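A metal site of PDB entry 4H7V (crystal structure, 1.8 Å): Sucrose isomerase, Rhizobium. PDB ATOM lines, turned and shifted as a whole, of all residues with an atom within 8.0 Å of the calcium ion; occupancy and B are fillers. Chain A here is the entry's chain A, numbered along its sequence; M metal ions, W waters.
Within 4 Å of the calcium ion: Asp 22, Asn 24, Asp 26, Ile 28 and Asp 30.
The nearest printed residue that does not touch the calcium ion is Thr 23 (4.3 Å).
OD2 of Asp 22 lies within hydrogen-bond range of N of Gly 27 (2.8 Å).
The side-chain carboxylate (OD2) of Asp 22 is in hydrogen-bond range of the backbone NH (N) of Gly 25 (3.3 Å).
OD2 of Asp 22 lies within hydrogen-bond range of OG1 of Thr 432 (2.7 Å).
The backbone carbonyl oxygen of Phe 431 lies within hydrogen-bond range of the backbone NH of Asp 22 (2.9 Å).
The side-chain carboxylate (OD1) of Asp 30 sits at hydrogen-bond distance from the side-chain hydroxyl (OG1) of Thr 23 (2.6 Å).
The backbone carbonyl oxygen of Lys 21 is in hydrogen-bond range of the backbone NH of Asp 30, at 3.0 Å.
OD1 of Asp 30 is in hydrogen-bond range of N of Gly 33 (3.0 Å).
Water W2 bridges ND2 of Asn 24 (3.2 Å) and O of Glu 75 (3.3 Å).
Water W1 lies within hydrogen-bond range of the backbone carbonyl oxygen (O) of Glu 75 (2.4 Å) and the side-chain carboxylate (OD2) of Asp 26 (2.7 Å).
The calcium ion is bound by the side-chain carboxylate (OD1) of Asp 22 (2.3 Å), the side-chain carboxylate (OD1) of Asp 26 (2.3 Å), the side-chain amide oxygen (OD1) of Asn 24 (2.3 Å), the side-chain carboxylate (OD2) of Asp 30 (2.4 Å), water W1 (2.4 Å), the backbone carbonyl oxygen (O) of Ile 28 (2.4 Å) and water W2 (2.4 Å).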
ATOM      1  N   PRO A  17      21.530  10.320  12.299  1.00  0.00           N
ATOM      2  CA  PRO A  17      21.253  11.715  11.897  1.00  0.00           C
ATOM      3  C   PRO A  17      20.029  12.282  12.634  1.00  0.00           C
ATOM      4  O   PRO A  17      20.008  13.463  12.971  1.00  0.00           O
ATOM      5  CB  PRO A  17      20.943  11.587  10.416  1.00  0.00           C
ATOM      6  CG  PRO A  17      21.797  10.437   9.972  1.00  0.00           C
ATOM      7  CD  PRO A  17      21.665   9.440  11.127  1.00  0.00           C
ATOM      8  N   ARG A  18      19.046  11.449  12.908  1.00  0.00           N
ATOM      9  CA  ARG A  18      17.826  11.851  13.618  1.00  0.00           C
ATOM     10  C   ARG A  18      18.120  12.551  14.959  1.00  0.00           C
ATOM     11  O   ARG A  18      17.319  13.398  15.429  1.00  0.00           O
ATOM     12  CB  ARG A  18      16.970  10.604  13.859  1.00  0.00           C
ATOM     13  CG  ARG A  18      15.553  10.888  14.168  1.00  0.00           C
ATOM     14  CD  ARG A  18      14.727   9.607  14.318  1.00  0.00           C
ATOM     15  NE  ARG A  18      13.401   9.978  14.751  1.00  0.00           N
ATOM     16  CZ  ARG A  18      12.353  10.139  13.948  1.00  0.00           C
ATOM     17  NH1 ARG A  18      12.446   9.905  12.640  1.00  0.00           N
ATOM     18  NH2 ARG A  18      11.174  10.508  14.463  1.00  0.00           N
ATOM     19  N   LYS A  21      22.112  16.624  14.956  1.00  0.00           N
ATOM     20  CA  LYS A  21      21.906  18.104  15.008  1.00  0.00           C
ATOM     21  C   LYS A  21      20.733  18.566  14.178  1.00  0.00           C
ATOM     22  O   LYS A  21      20.661  18.296  12.959  1.00  0.00           O
ATOM     23  CB  LYS A  21      23.162  18.877  14.585  1.00  0.00           C
ATOM     24  CG  LYS A  21      22.997  20.457  14.556  1.00  0.00           C
ATOM     25  CD  LYS A  21      22.870  20.981  16.007  1.00  0.00           C
ATOM     26  CE  LYS A  21      22.574  22.498  16.139  1.00  0.00           C
ATOM     27  NZ  LYS A  21      22.806  23.267  14.872  1.00  0.00           N
ATOM     28  N   ASP A  22      19.786  19.242  14.814  1.00  0.00           N
ATOM     29  CA  ASP A  22      18.629  19.756  14.072  1.00  0.00           C
ATOM     30  C   ASP A  22      18.904  21.203  13.676  1.00  0.00           C
ATOM     31  O   ASP A  22      19.499  21.978  14.436  1.00  0.00           O
ATOM     32  CB  ASP A  22      17.386  19.656  14.939  1.00  0.00           C
ATOM     33  CG  ASP A  22      16.138  20.309  14.324  1.00  0.00           C
ATOM     34  OD1 ASP A  22      16.039  20.479  13.097  1.00  0.00           O
ATOM     35  OD2 ASP A  22      15.213  20.620  15.112  1.00  0.00           O
ATOM     36  N   THR A  23      18.493  21.596  12.477  1.00  0.00           N
ATOM     37  CA  THR A  23      18.734  22.971  12.063  1.00  0.00           C
ATOM     38  C   THR A  23      17.467  23.714  11.649  1.00  0.00           C
ATOM     39  O   THR A  23      17.543  24.893  11.278  1.00  0.00           O
ATOM     40  CB  THR A  23      19.701  23.055  10.863  1.00  0.00           C
ATOM     41  OG1 THR A  23      19.212  22.216   9.802  1.00  0.00           O
ATOM     42  CG2 THR A  23      21.079  22.600  11.227  1.00  0.00           C
ATOM     43  N   ASN A  24      16.291  23.073  11.725  1.00  0.00           N
ATOM     44  CA  ASN A  24      15.051  23.770  11.392  1.00  0.00           C
ATOM     45  C   ASN A  24      13.942  23.676  12.466  1.00  0.00           C
ATOM     46  O   ASN A  24      12.755  23.764  12.171  1.00  0.00           O
ATOM     47  CB  ASN A  24      14.530  23.339  10.023  1.00  0.00           C
ATOM     48  CG  ASN A  24      13.949  21.919  10.046  1.00  0.00           C
ATOM     49  OD1 ASN A  24      14.266  21.129  10.928  1.00  0.00           O
ATOM     50  ND2 ASN A  24      13.080  21.620   9.093  1.00  0.00           N
ATOM     51  N   GLY A  25      14.321  23.453  13.708  1.00  0.00           N
ATOM     52  CA  GLY A  25      13.364  23.465  14.810  1.00  0.00           C
ATOM     53  C   GLY A  25      12.244  22.455  14.838  1.00  0.00           C
ATOM     54  O   GLY A  25      11.330  22.592  15.658  1.00  0.00           O
ATOM     55  N   ASP A  26      12.276  21.412  13.991  1.00  0.00           N
ATOM     56  CA  ASP A  26      11.255  20.397  14.057  1.00  0.00           C
ATOM     57  C   ASP A  26      11.615  19.290  15.056  1.00  0.00           C
ATOM     58  O   ASP A  26      10.859  18.331  15.197  1.00  0.00           O
ATOM     59  CB  ASP A  26      10.966  19.803  12.671  1.00  0.00           C
ATOM     60  CG  ASP A  26      12.120  18.910  12.157  1.00  0.00           C
ATOM     61  OD1 ASP A  26      13.241  18.986  12.672  1.00  0.00           O
ATOM     62  OD2 ASP A  26      11.880  18.122  11.224  1.00  0.00           O
ATOM     63  N   GLY A  27      12.747  19.440  15.735  1.00  0.00           N
ATOM     64  CA  GLY A  27      13.175  18.501  16.761  1.00  0.00           C
ATOM     65  C   GLY A  27      13.804  17.199  16.242  1.00  0.00           C
ATOM     66  O   GLY A  27      14.128  16.261  17.017  1.00  0.00           O
ATOM     67  N   ILE A  28      13.985  17.112  14.936  1.00  0.00           N
ATOM     68  CA  ILE A  28      14.627  15.912  14.369  1.00  0.00           C
ATOM     69  C   ILE A  28      15.922  16.340  13.712  1.00  0.00           C
ATOM     70  O   ILE A  28      15.934  17.337  13.013  1.00  0.00           O
ATOM     71  CB  ILE A  28      13.728  15.274  13.325  1.00  0.00           C
ATOM     72  CG1 ILE A  28      12.452  14.776  13.989  1.00  0.00           C
ATOM     73  CG2 ILE A  28      14.475  14.161  12.635  1.00  0.00           C
ATOM     74  CD1 ILE A  28      11.333  14.442  13.013  1.00  0.00           C
ATOM     75  N   GLY A  29      17.039  15.630  13.957  1.00  0.00           N
ATOM     76  CA  GLY A  29      18.289  15.980  13.303  1.00  0.00           C
ATOM     77  C   GLY A  29      18.216  15.863  11.792  1.00  0.00           C
ATOM     78  O   GLY A  29      17.337  15.161  11.256  1.00  0.00           O
ATOM     79  N   ASP A  30      19.158  16.507  11.105  1.00  0.00           N
ATOM     80  CA  ASP A  30      19.069  16.549   9.632  1.00  0.00           C
ATOM     81  C   ASP A  30      20.467  16.735   9.013  1.00  0.00           C
ATOM     82  O   ASP A  30      21.477  16.863   9.735  1.00  0.00           O
ATOM     83  CB  ASP A  30      18.085  17.671   9.220  1.00  0.00           C
ATOM     84  CG  ASP A  30      18.325  18.989   9.983  1.00  0.00           C
ATOM     85  OD1 ASP A  30      19.427  19.576   9.827  1.00  0.00           O
ATOM     86  OD2 ASP A  30      17.439  19.454  10.750  1.00  0.00           O
ATOM     87  N   PHE A  31      20.517  16.683   7.669  1.00  0.00           N
ATOM     88  CA  PHE A  31      21.761  16.715   6.924  1.00  0.00           C
ATOM     89  C   PHE A  31      22.472  18.065   7.077  1.00  0.00           C
ATOM     90  O   PHE A  31      23.694  18.088   7.192  1.00  0.00           O
ATOM     91  CB  PHE A  31      21.473  16.479   5.453  1.00  0.00           C
ATOM     92  CG  PHE A  31      21.332  15.010   5.102  1.00  0.00           C
ATOM     93  CD1 PHE A  31      22.041  14.066   5.814  1.00  0.00           C
ATOM     94  CD2 PHE A  31      20.514  14.604   4.074  1.00  0.00           C
ATOM     95  CE1 PHE A  31      21.938  12.723   5.509  1.00  0.00           C
ATOM     96  CE2 PHE A  31      20.399  13.245   3.757  1.00  0.00           C
ATOM     97  CZ  PHE A  31      21.118  12.318   4.471  1.00  0.00           C
ATOM     98  N   LYS A  32      21.724  19.162   7.089  1.00  0.00           N
ATOM     99  CA  LYS A  32      22.353  20.487   7.310  1.00  0.00           C
ATOM    100  C   LYS A  32      23.033  20.563   8.682  1.00  0.00           C
ATOM    101  O   LYS A  32      24.138  21.100   8.824  1.00  0.00           O
ATOM    102  CB  LYS A  32      21.332  21.621   7.172  1.00  0.00           C
ATOM    103  N   GLY A  33      22.383  19.951   9.683  1.00  0.00           N
ATOM    104  CA  GLY A  33      22.974  19.874  11.011  1.00  0.00           C
ATOM    105  C   GLY A  33      24.258  19.069  11.045  1.00  0.00           C
ATOM    106  O   GLY A  33      25.280  19.507  11.591  1.00  0.00           O
ATOM    107  N   LYS A  74      12.678  12.678   3.880  1.00  0.00           N
ATOM    108  CA  LYS A  74      12.193  14.061   3.893  1.00  0.00           C
ATOM    109  C   LYS A  74      12.697  14.819   5.123  1.00  0.00           C
ATOM    110  O   LYS A  74      13.119  15.976   5.028  1.00  0.00           O
ATOM    111  CB  LYS A  74      10.650  14.100   3.822  1.00  0.00           C
ATOM    112  N   GLU A  75      12.670  14.146   6.264  1.00  0.00           N
ATOM    113  CA  GLU A  75      13.064  14.768   7.518  1.00  0.00           C
ATOM    114  C   GLU A  75      14.546  15.184   7.497  1.00  0.00           C
ATOM    115  O   GLU A  75      14.917  16.122   8.202  1.00  0.00           O
ATOM    116  CB  GLU A  75      12.838  13.794   8.668  1.00  0.00           C
ATOM    117  CG  GLU A  75      11.392  13.649   9.126  1.00  0.00           C
ATOM    118  CD  GLU A  75      10.521  12.809   8.209  1.00  0.00           C
ATOM    119  OE1 GLU A  75      11.094  12.084   7.360  1.00  0.00           O
ATOM    120  OE2 GLU A  75       9.268  12.879   8.338  1.00  0.00           O
ATOM    121  N   TYR A  76      15.388  14.514   6.703  1.00  0.00           N
ATOM    122  CA  TYR A  76      16.840  14.896   6.742  1.00  0.00           C
ATOM    123  C   TYR A  76      17.197  15.946   5.709  1.00  0.00           C
ATOM    124  O   TYR A  76      18.296  16.564   5.773  1.00  0.00           O
ATOM    125  CB  TYR A  76      17.795  13.709   6.575  1.00  0.00           C
ATOM    126  CG  TYR A  76      17.595  12.613   7.580  1.00  0.00           C
ATOM    127  CD1 TYR A  76      17.029  12.867   8.842  1.00  0.00           C
ATOM    128  CD2 TYR A  76      17.972  11.317   7.289  1.00  0.00           C
ATOM    129  CE1 TYR A  76      16.824  11.840   9.756  1.00  0.00           C
ATOM    130  CE2 TYR A  76      17.787  10.301   8.212  1.00  0.00           C
ATOM    131  CZ  TYR A  76      17.222  10.570   9.436  1.00  0.00           C
ATOM    132  OH  TYR A  76      17.001   9.542  10.332  1.00  0.00           O
ATOM    133  N   GLY A  77      16.310  16.162   4.750  1.00  0.00           N
ATOM    134  CA  GLY A  77      16.631  17.127   3.728  1.00  0.00           C
ATOM    135  C   GLY A  77      16.335  16.620   2.348  1.00  0.00           C
ATOM    136  O   GLY A  77      15.488  15.742   2.146  1.00  0.00           O
ATOM    137  N   PHE A 431      20.848  20.968  20.672  1.00  0.00           N
ATOM    138  CA  PHE A 431      20.537  20.074  19.548  1.00  0.00           C
ATOM    139  C   PHE A 431      19.414  20.637  18.676  1.00  0.00           C
ATOM    140  O   PHE A 431      19.435  20.487  17.454  1.00  0.00           O
ATOM    141  CB  PHE A 431      20.186  18.676  20.054  1.00  0.00           C
ATOM    142  CG  PHE A 431      19.299  17.892  19.127  1.00  0.00           C
ATOM    143  CD1 PHE A 431      19.828  17.223  18.048  1.00  0.00           C
ATOM    144  CD2 PHE A 431      17.938  17.771  19.383  1.00  0.00           C
ATOM    145  CE1 PHE A 431      19.061  16.524  17.221  1.00  0.00           C
ATOM    146  CE2 PHE A 431      17.135  17.012  18.551  1.00  0.00           C
ATOM    147  CZ  PHE A 431      17.716  16.384  17.442  1.00  0.00           C
ATOM    148  N   THR A 432      18.433  21.275  19.310  1.00  0.00           N
ATOM    149  CA  THR A 432      17.297  21.824  18.571  1.00  0.00           C
ATOM    150  C   THR A 432      16.827  23.123  19.223  1.00  0.00           C
ATOM    151  O   THR A 432      17.122  23.367  20.397  1.00  0.00           O
ATOM    152  CB  THR A 432      16.114  20.872  18.485  1.00  0.00           C
ATOM    153  OG1 THR A 432      15.098  21.460  17.655  1.00  0.00           O
ATOM    154  CG2 THR A 432      15.533  20.599  19.848  1.00  0.00           C
HETATM  155 CA    CA M   1      15.219  19.078  11.469  1.00  0.00          CA
HETATM  156  O   HOH W   1      14.233  17.276  10.248  1.00  0.00           O
HETATM  157  O   HOH W   2      15.230  19.265   9.035  1.00  0.00           O
